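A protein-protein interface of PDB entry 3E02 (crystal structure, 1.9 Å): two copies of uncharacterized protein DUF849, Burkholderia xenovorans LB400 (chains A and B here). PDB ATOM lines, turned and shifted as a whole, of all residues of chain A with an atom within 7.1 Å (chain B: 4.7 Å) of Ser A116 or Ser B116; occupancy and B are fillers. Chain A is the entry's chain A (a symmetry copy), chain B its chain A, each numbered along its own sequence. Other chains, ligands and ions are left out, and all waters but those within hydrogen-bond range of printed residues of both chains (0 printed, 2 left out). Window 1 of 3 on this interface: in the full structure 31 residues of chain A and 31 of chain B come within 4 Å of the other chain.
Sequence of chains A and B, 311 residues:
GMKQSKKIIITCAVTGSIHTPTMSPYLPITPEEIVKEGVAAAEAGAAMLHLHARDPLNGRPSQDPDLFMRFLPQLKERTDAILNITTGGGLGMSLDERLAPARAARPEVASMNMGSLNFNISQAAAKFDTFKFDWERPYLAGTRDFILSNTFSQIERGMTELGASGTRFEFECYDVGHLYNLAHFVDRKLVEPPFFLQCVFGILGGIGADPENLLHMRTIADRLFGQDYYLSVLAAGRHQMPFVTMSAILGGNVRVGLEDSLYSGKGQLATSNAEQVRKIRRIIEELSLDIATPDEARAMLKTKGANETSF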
ATOM      1  N   ASN A 113      27.991  -8.139 -34.797  1.00  0.00           N
ATOM      2  CA  ASN A 113      27.743  -8.582 -33.425  1.00  0.00           C
ATOM      3  C   ASN A 113      27.169  -9.999 -33.465  1.00  0.00           C
ATOM      4  O   ASN A 113      26.165 -10.232 -34.143  1.00  0.00           O
ATOM      5  CB  ASN A 113      26.852  -7.573 -32.734  1.00  0.00           C
ATOM      6  CG  ASN A 113      27.531  -6.212 -32.622  1.00  0.00           C
ATOM      7  OD1 ASN A 113      28.535  -6.086 -31.941  1.00  0.00           O
ATOM      8  ND2 ASN A 113      27.016  -5.209 -33.348  1.00  0.00           N
ATOM      9  N   MET A 114      27.830 -10.930 -32.762  1.00  0.00           N
ATOM     10  CA  MET A 114      27.517 -12.379 -32.869  1.00  0.00           C
ATOM     11  C   MET A 114      26.467 -12.983 -31.939  1.00  0.00           C
ATOM     12  O   MET A 114      26.296 -14.199 -31.902  1.00  0.00           O
ATOM     13  CB  MET A 114      28.824 -13.190 -32.856  1.00  0.00           C
ATOM     14  CG  MET A 114      29.663 -13.024 -34.115  1.00  0.00           C
ATOM     15  SD  MET A 114      28.667 -13.373 -35.753  1.00  0.00           S
ATOM     16  CE  MET A 114      28.009 -15.034 -35.356  1.00  0.00           C
ATOM     17  N   GLY A 115      25.718 -12.150 -31.241  1.00  0.00           N
ATOM     18  CA  GLY A 115      24.646 -12.667 -30.400  1.00  0.00           C
ATOM     19  C   GLY A 115      23.876 -11.569 -29.732  1.00  0.00           C
ATOM     20  O   GLY A 115      24.319 -10.418 -29.714  1.00  0.00           O
ATOM     21  N   SER A 116      22.706 -11.922 -29.221  1.00  0.00           N
ATOM     22  CA  SER A 116      21.854 -10.975 -28.510  1.00  0.00           C
ATOM     23  C   SER A 116      22.241 -11.022 -27.047  1.00  0.00           C
ATOM     24  O   SER A 116      22.462 -12.107 -26.485  1.00  0.00           O
ATOM     25  CB  SER A 116      20.375 -11.314 -28.684  1.00  0.00           C
ATOM     26  OG  SER A 116      19.998 -11.302 -30.049  1.00  0.00           O
ATOM     27  N   LEU A 117      22.381  -9.858 -26.426  1.00  0.00           N
ATOM     28  CA  LEU A 117      22.680  -9.792 -25.005  1.00  0.00           C
ATOM     29  C   LEU A 117      22.129  -8.544 -24.347  1.00  0.00           C
ATOM     30  O   LEU A 117      21.962  -7.511 -25.006  1.00  0.00           O
ATOM     31  CB  LEU A 117      24.204  -9.801 -24.768  1.00  0.00           C
ATOM     32  CG  LEU A 117      25.068  -8.617 -25.267  1.00  0.00           C
ATOM     33  CD1 LEU A 117      26.341  -8.439 -24.437  1.00  0.00           C
ATOM     34  CD2 LEU A 117      25.393  -8.746 -26.758  1.00  0.00           C
ATOM     35  N   ASN A 118      21.923  -8.631 -23.036  1.00  0.00           N
ATOM     36  CA  ASN A 118      21.670  -7.438 -22.220  1.00  0.00           C
ATOM     37  C   ASN A 118      22.911  -6.544 -22.392  1.00  0.00           C
ATOM     38  O   ASN A 118      24.028  -7.054 -22.475  1.00  0.00           O
ATOM     39  CB  ASN A 118      21.517  -7.786 -20.740  1.00  0.00           C
ATOM     40  CG  ASN A 118      20.240  -8.535 -20.437  1.00  0.00           C
ATOM     41  OD1 ASN A 118      19.318  -8.575 -21.255  1.00  0.00           O
ATOM     42  ND2 ASN A 118      20.167  -9.116 -19.241  1.00  0.00           N
ATOM     43  N   PHE A 146      17.369  -2.988 -21.885  1.00  0.00           N
ATOM     44  CA  PHE A 146      17.795  -3.054 -23.277  1.00  0.00           C
ATOM     45  C   PHE A 146      18.548  -4.335 -23.612  1.00  0.00           C
ATOM     46  O   PHE A 146      19.356  -4.804 -22.811  1.00  0.00           O
ATOM     47  CB  PHE A 146      18.701  -1.868 -23.579  1.00  0.00           C
ATOM     48  CG  PHE A 146      19.274  -1.857 -24.972  1.00  0.00           C
ATOM     49  CD1 PHE A 146      18.464  -1.603 -26.074  1.00  0.00           C
ATOM     50  CD2 PHE A 146      20.631  -2.086 -25.186  1.00  0.00           C
ATOM     51  CE1 PHE A 146      19.002  -1.598 -27.369  1.00  0.00           C
ATOM     52  CE2 PHE A 146      21.168  -2.074 -26.468  1.00  0.00           C
ATOM     53  CZ  PHE A 146      20.347  -1.824 -27.561  1.00  0.00           C
ATOM     54  N   ILE A 147      18.290  -4.845 -24.820  1.00  0.00           N
ATOM     55  CA  ILE A 147      18.974  -6.004 -25.389  1.00  0.00           C
ATOM     56  C   ILE A 147      19.596  -5.535 -26.705  1.00  0.00           C
ATOM     57  O   ILE A 147      18.895  -4.964 -27.547  1.00  0.00           O
ATOM     58  CB  ILE A 147      17.997  -7.166 -25.699  1.00  0.00           C
ATOM     59  CG1 ILE A 147      17.273  -7.641 -24.429  1.00  0.00           C
ATOM     60  CG2 ILE A 147      18.751  -8.351 -26.350  1.00  0.00           C
ATOM     61  CD1 ILE A 147      16.104  -8.580 -24.704  1.00  0.00           C
ATOM     62  N   LEU A 148      20.899  -5.745 -26.872  1.00  0.00           N
ATOM     63  CA  LEU A 148      21.567  -5.483 -28.150  1.00  0.00           C
ATOM     64  C   LEU A 148      21.167  -6.718 -28.974  1.00  0.00           C
ATOM     65  O   LEU A 148      21.678  -7.816 -28.750  1.00  0.00           O
ATOM     66  CB  LEU A 148      23.082  -5.368 -27.999  1.00  0.00           C
ATOM     67  CG  LEU A 148      23.846  -5.082 -29.300  1.00  0.00           C
ATOM     68  CD1 LEU A 148      23.501  -3.677 -29.824  1.00  0.00           C
ATOM     69  CD2 LEU A 148      25.337  -5.230 -29.092  1.00  0.00           C
ATOM     70  N   SER A 149      20.222  -6.534 -29.886  1.00  0.00           N
ATOM     71  CA  SER A 149      19.623  -7.642 -30.644  1.00  0.00           C
ATOM     72  C   SER A 149      20.447  -8.100 -31.834  1.00  0.00           C
ATOM     73  O   SER A 149      20.766  -7.301 -32.679  1.00  0.00           O
ATOM     74  CB  SER A 149      18.237  -7.237 -31.148  1.00  0.00           C
ATOM     75  OG  SER A 149      17.612  -8.313 -31.853  1.00  0.00           O
ATOM     76  N   ASN A 150      20.783  -9.392 -31.900  1.00  0.00           N
ATOM     77  CA  ASN A 150      21.449  -9.997 -33.069  1.00  0.00           C
ATOM     78  C   ASN A 150      20.986 -11.456 -33.145  1.00  0.00           C
ATOM     79  O   ASN A 150      21.720 -12.367 -32.814  1.00  0.00           O
ATOM     80  CB  ASN A 150      22.980  -9.923 -32.970  1.00  0.00           C
ATOM     81  CG  ASN A 150      23.484  -8.522 -32.821  1.00  0.00           C
ATOM     82  OD1 ASN A 150      23.481  -7.782 -33.788  1.00  0.00           O
ATOM     83  ND2 ASN A 150      23.904  -8.137 -31.605  1.00  0.00           N
ATOM     84  N   THR A 151      19.742 -11.656 -33.579  1.00  0.00           N
ATOM     85  CA  THR A 151      19.175 -12.998 -33.692  1.00  0.00           C
ATOM     86  C   THR A 151      19.867 -13.741 -34.828  1.00  0.00           C
ATOM     87  O   THR A 151      20.556 -13.120 -35.645  1.00  0.00           O
ATOM     88  CB  THR A 151      17.658 -12.981 -33.925  1.00  0.00           C
ATOM     89  OG1 THR A 151      17.380 -12.439 -35.216  1.00  0.00           O
ATOM     90  CG2 THR A 151      16.917 -12.190 -32.839  1.00  0.00           C
ATOM     91  N   PHE A 152      19.712 -15.065 -34.876  1.00  0.00           N
ATOM     92  CA  PHE A 152      20.290 -15.842 -35.979  1.00  0.00           C
ATOM     93  C   PHE A 152      19.795 -15.338 -37.348  1.00  0.00           C
ATOM     94  O   PHE A 152      20.580 -15.231 -38.276  1.00  0.00           O
ATOM     95  CB  PHE A 152      20.068 -17.345 -35.783  1.00  0.00           C
ATOM     96  CG  PHE A 152      20.982 -17.935 -34.756  1.00  0.00           C
ATOM     97  CD1 PHE A 152      20.643 -17.933 -33.408  1.00  0.00           C
ATOM     98  CD2 PHE A 152      22.211 -18.458 -35.133  1.00  0.00           C
ATOM     99  CE1 PHE A 152      21.507 -18.475 -32.454  1.00  0.00           C
ATOM    100  CE2 PHE A 152      23.080 -18.996 -34.196  1.00  0.00           C
ATOM    101  CZ  PHE A 152      22.738 -19.003 -32.864  1.00  0.00           C
ATOM    102  N   GLN A 154      18.804 -12.201 -38.023  1.00  0.00           N
ATOM    103  CA  GLN A 154      19.435 -10.879 -38.207  1.00  0.00           C
ATOM    104  C   GLN A 154      20.890 -11.016 -38.652  1.00  0.00           C
ATOM    105  O   GLN A 154      21.327 -10.328 -39.577  1.00  0.00           O
ATOM    106  CB  GLN A 154      19.320 -10.026 -36.941  1.00  0.00           C
ATOM    107  CG  GLN A 154      17.901  -9.533 -36.684  1.00  0.00           C
ATOM    108  CD  GLN A 154      17.783  -8.710 -35.419  1.00  0.00           C
ATOM    109  OE1 GLN A 154      18.326  -9.058 -34.365  1.00  0.00           O
ATOM    110  NE2 GLN A 154      17.057  -7.605 -35.510  1.00  0.00           N
ATOM    111  N   ILE A 155      21.630 -11.916 -38.003  1.00  0.00           N
ATOM    112  CA  ILE A 155      23.038 -12.166 -38.355  1.00  0.00           C
ATOM    113  C   ILE A 155      23.139 -12.669 -39.795  1.00  0.00           C
ATOM    114  O   ILE A 155      23.945 -12.156 -40.574  1.00  0.00           O
ATOM    115  CB  ILE A 155      23.726 -13.146 -37.382  1.00  0.00           C
ATOM    116  CG1 ILE A 155      23.790 -12.538 -35.964  1.00  0.00           C
ATOM    117  CG2 ILE A 155      25.145 -13.459 -37.886  1.00  0.00           C
ATOM    118  CD1 ILE A 155      24.056 -13.565 -34.843  1.00  0.00           C
ATOM    119  N   HIS A 178      28.711 -16.716 -28.180  1.00  0.00           N
ATOM    120  CA  HIS A 178      28.912 -16.028 -29.466  1.00  0.00           C
ATOM    121  C   HIS A 178      29.873 -16.785 -30.382  1.00  0.00           C
ATOM    122  O   HIS A 178      29.723 -16.721 -31.602  1.00  0.00           O
ATOM    123  CB  HIS A 178      29.378 -14.598 -29.246  1.00  0.00           C
ATOM    124  CG  HIS A 178      28.349 -13.722 -28.598  1.00  0.00           C
ATOM    125  ND1 HIS A 178      28.328 -12.360 -28.779  1.00  0.00           N
ATOM    126  CD2 HIS A 178      27.252 -14.017 -27.859  1.00  0.00           C
ATOM    127  CE1 HIS A 178      27.319 -11.841 -28.099  1.00  0.00           C
ATOM    128  NE2 HIS A 178      26.644 -12.829 -27.539  1.00  0.00           N
ATOM    129  N   ASN A 181      27.772 -19.480 -31.798  1.00  0.00           N
ATOM    130  CA  ASN A 181      26.882 -18.825 -32.801  1.00  0.00           C
ATOM    131  C   ASN A 181      27.640 -18.650 -34.120  1.00  0.00           C
ATOM    132  O   ASN A 181      27.102 -18.965 -35.176  1.00  0.00           O
ATOM    133  CB  ASN A 181      26.373 -17.456 -32.314  1.00  0.00           C
ATOM    134  CG  ASN A 181      25.459 -17.553 -31.099  1.00  0.00           C
ATOM    135  OD1 ASN A 181      25.092 -18.650 -30.660  1.00  0.00           O
ATOM    136  ND2 ASN A 181      25.081 -16.388 -30.556  1.00  0.00           N
ATOM    137  N   GLY A 205      26.236  -7.427 -18.910  1.00  0.00           N
ATOM    138  CA  GLY A 205      25.403  -8.182 -19.834  1.00  0.00           C
ATOM    139  C   GLY A 205      26.276  -9.126 -20.663  1.00  0.00           C
ATOM    140  O   GLY A 205      25.773 -10.107 -21.186  1.00  0.00           O
ATOM    141  N   GLY B 115      19.813 -13.928 -18.116  1.00  0.00           N
ATOM    142  CA  GLY B 115      20.246 -13.050 -19.194  1.00  0.00           C
ATOM    143  C   GLY B 115      19.451 -13.266 -20.448  1.00  0.00           C
ATOM    144  O   GLY B 115      18.734 -14.262 -20.568  1.00  0.00           O
ATOM    145  N   SER B 116      19.551 -12.309 -21.358  1.00  0.00           N
ATOM    146  CA  SER B 116      18.866 -12.388 -22.643  1.00  0.00           C
ATOM    147  C   SER B 116      19.795 -13.084 -23.615  1.00  0.00           C
ATOM    148  O   SER B 116      21.005 -12.807 -23.642  1.00  0.00           O
ATOM    149  CB  SER B 116      18.489 -11.002 -23.162  1.00  0.00           C
ATOM    150  OG  SER B 116      17.641 -10.322 -22.255  1.00  0.00           O
ATOM    151  N   LEU B 117      19.264 -14.028 -24.381  1.00  0.00           N
ATOM    152  CA  LEU B 117      20.052 -14.707 -25.397  1.00  0.00           C
ATOM    153  C   LEU B 117      19.218 -15.173 -26.572  1.00  0.00           C
ATOM    154  O   LEU B 117      18.019 -15.434 -26.422  1.00  0.00           O
ATOM    155  CB  LEU B 117      20.747 -15.950 -24.805  1.00  0.00           C
ATOM    156  CG  LEU B 117      19.895 -17.141 -24.301  1.00  0.00           C
ATOM    157  CD1 LEU B 117      20.656 -18.467 -24.372  1.00  0.00           C
ATOM    158  CD2 LEU B 117      19.353 -16.890 -22.892  1.00  0.00           C
ATOM    159  N   ASN B 118      19.880 -15.344 -27.713  1.00  0.00           N
ATOM    160  CA  ASN B 118      19.280 -16.055 -28.847  1.00  0.00           C
ATOM    161  C   ASN B 118      18.962 -17.470 -28.331  1.00  0.00           C
ATOM    162  O   ASN B 118      19.730 -18.023 -27.544  1.00  0.00           O
ATOM    163  CB  ASN B 118      20.251 -16.169 -30.022  1.00  0.00           C
ATOM    164  CG  ASN B 118      20.512 -14.846 -30.704  1.00  0.00           C
ATOM    165  OD1 ASN B 118      19.781 -13.873 -30.503  1.00  0.00           O
ATOM    166  ND2 ASN B 118      21.547 -14.808 -31.541  1.00  0.00           N
ATOM    167  N   ILE B 147      14.685 -14.147 -29.226  1.00  0.00           N
ATOM    168  CA  ILE B 147      15.545 -13.860 -28.079  1.00  0.00           C
ATOM    169  C   ILE B 147      14.740 -14.225 -26.832  1.00  0.00           C
ATOM    170  O   ILE B 147      13.605 -13.760 -26.675  1.00  0.00           O
ATOM    171  CB  ILE B 147      15.923 -12.359 -27.993  1.00  0.00           C
ATOM    172  CG1 ILE B 147      16.672 -11.898 -29.253  1.00  0.00           C
ATOM    173  CG2 ILE B 147      16.787 -12.087 -26.737  1.00  0.00           C
ATOM    174  CD1 ILE B 147      16.824 -10.385 -29.359  1.00  0.00           C
ATOM    175  N   LEU B 148      15.300 -15.067 -25.969  1.00  0.00           N
ATOM    176  CA  LEU B 148      14.692 -15.361 -24.668  1.00  0.00           C
ATOM    177  C   LEU B 148      15.077 -14.118 -23.850  1.00  0.00           C
ATOM    178  O   LEU B 148      16.232 -13.961 -23.452  1.00  0.00           O
ATOM    179  CB  LEU B 148      15.243 -16.643 -24.049  1.00  0.00           C
ATOM    180  CG  LEU B 148      14.639 -17.019 -22.688  1.00  0.00           C
ATOM    181  CD1 LEU B 148      13.155 -17.392 -22.846  1.00  0.00           C
ATOM    182  CD2 LEU B 148      15.415 -18.151 -22.049  1.00  0.00           C
ATOM    183  N   SER B 149      14.116 -13.227 -23.651  1.00  0.00           N
ATOM    184  CA  SER B 149      14.363 -11.921 -23.024  1.00  0.00           C
ATOM    185  C   SER B 149      14.414 -11.956 -21.507  1.00  0.00           C
ATOM    186  O   SER B 149      13.482 -12.409 -20.891  1.00  0.00           O
ATOM    187  CB  SER B 149      13.276 -10.930 -23.443  1.00  0.00           C
ATOM    188  OG  SER B 149      13.515  -9.637 -22.882  1.00  0.00           O
ATOM    189  N   ASN B 150      15.505 -11.470 -20.908  1.00  0.00           N
ATOM    190  CA  ASN B 150      15.623 -11.307 -19.446  1.00  0.00           C
ATOM    191  C   ASN B 150      16.541 -10.105 -19.200  1.00  0.00           C
ATOM    192  O   ASN B 150      17.689 -10.256 -18.829  1.00  0.00           O
ATOM    193  CB  ASN B 150      16.186 -12.562 -18.763  1.00  0.00           C
ATOM    194  CG  ASN B 150      15.364 -13.784 -19.030  1.00  0.00           C
ATOM    195  OD1 ASN B 150      14.295 -13.919 -18.465  1.00  0.00           O
ATOM    196  ND2 ASN B 150      15.845 -14.678 -19.910  1.00  0.00           N
ATOM    197  N   THR B 151      16.011  -8.904 -19.428  1.00  0.00           N
ATOM    198  CA  THR B 151      16.781  -7.677 -19.240  1.00  0.00           C
ATOM    199  C   THR B 151      17.033  -7.466 -17.752  1.00  0.00           C
ATOM    200  O   THR B 151      16.390  -8.113 -16.918  1.00  0.00           O
ATOM    201  CB  THR B 151      16.085  -6.444 -19.833  1.00  0.00           C
ATOM    202  OG1 THR B 151      14.901  -6.161 -19.088  1.00  0.00           O
ATOM    203  CG2 THR B 151      15.754  -6.630 -21.319  1.00  0.00           C
ATOM    204  N   HIS B 178      26.029 -14.561 -17.738  1.00  0.00           N
ATOM    205  CA  HIS B 178      24.912 -14.731 -16.794  1.00  0.00           C
ATOM    206  C   HIS B 178      25.386 -14.784 -15.341  1.00  0.00           C
ATOM    207  O   HIS B 178      24.656 -14.352 -14.451  1.00  0.00           O
ATOM    208  CB  HIS B 178      24.091 -15.961 -17.146  1.00  0.00           C
ATOM    209  CG  HIS B 178      23.362 -15.845 -18.451  1.00  0.00           C
ATOM    210  ND1 HIS B 178      22.207 -16.543 -18.709  1.00  0.00           N
ATOM    211  CD2 HIS B 178      23.561 -15.043 -19.526  1.00  0.00           C
ATOM    212  CE1 HIS B 178      21.779 -16.249 -19.925  1.00  0.00           C
ATOM    213  NE2 HIS B 178      22.579 -15.334 -20.439  1.00  0.00           N
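Among the printed residues, pairs that only touch across the chains: Gly A115 with Asn B118, Ser A116 with Leu B117, Ser A116 with Ile B147, Leu A117 with Ser B116, Asn A118 with Gly B115, Asn A118 with Thr B151, Ile A147 with Ser B116, Ile A147 with Ser B149, Ile A147 with Thr B151, Ser A149 with Ile B147, Thr A151 with Asn B118, Thr A151 with Ile B147, Phe A152 with Asn B118 and Asn A181 with Asn B118.
Gly A115 touches Asn B118, and with the chains exchanged Asn A118 touches Gly B115. Ser B116 touches its own counterpart, Ser A116. Asn A118 touches Thr B151, and with the chains exchanged Thr A151 touches Asn B118. Ile A147 touches Thr B151, and with the chains exchanged Thr A151 touches Ile B147. Positions printed for both chains: 115, 116, 117, 118, 147, 148, 149, 150, 151 and 178. Of the 19 pairs that touch across the chains among the printed residues, 17 have their exchanged pair printed and touching as well.
Of the 18 printed residues of chain A, 10 touch a printed residue of chain B. Printed residues of chain A that touch a printed residue of chain B: Gly A115, Ser A116, Leu A117, Asn A118, Ile A147, Ser A149, Asn A150, Thr A151, Phe A152 and Asn A181. Hydrophobic or aromatic side chains of chain A that line the printed part of chain B: Ile A147 and Phe A152. Of the 10 printed residues of chain B, 8 touch a printed residue of chain A. Along chain B the printed residues that touch a printed residue of chain A span positions 115 to 151. Among the printed residues, 19 pairs touch across the chains.
Of the printed residues of chain B, Asn A150 touches Asn B118 (2.8 Å). Of the printed residues of chain B, Thr A151 touches Asn B118 (3.4 Å) and Ile B147 (3.6 Å). Printed residues of chain B within 4 Å of Asn A181: Asn B118 (3.99 Å). Printed residues of chain A within 4 Å of Gly B115: Asn A118 (3.9 Å). Printed residues of chain A within 4 Å of Ile B147: Ser A116 (3.4 Å), Ser A149 (3.3 Å) and Thr A151 (3.6 Å). The nearest residue of chain A that does not touch Ser B116 is Phe A146 (5.8 Å). The nearest printed residue of chain A that does not touch Gly B115 is Gly A205 (6.6 Å).
OG of Ser B116 is in hydrogen-bond range of OD1 of Asn A118 (2.6 Å). The side-chain amide oxygen (OD1) of Asn B118 sits at hydrogen-bond distance from the side-chain hydroxyl (OG) of Ser A116. The backbone carbonyl oxygen (O) of Asn A150 lies within hydrogen-bond range of the side-chain amide nitrogen (ND2) of Asn B118 (2.8 Å). ND2 of Asn A118 lies within hydrogen-bond range of O of Asn B150 (2.8 Å). O of Ser A116 sits close to O of Ser B116, at 3.3 Å.
O of Gly B115 lies within hydrogen-bond range of ND2 of Asn B150 (3.0 Å). OG of Ser B116 is in hydrogen-bond range of N of Asn B150 (2.8 Å). The backbone carbonyl oxygen (O) of Leu B117 sits at hydrogen-bond distance from the backbone NH (N) of Leu B148. ND2 of Asn A181 sits at hydrogen-bond distance from O of Met A114, at 2.8 Å. N of Asn A150 is in hydrogen-bond range of OG of Ser A116. OE1 of Gln A154 lies within hydrogen-bond range of N of Asn A150.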
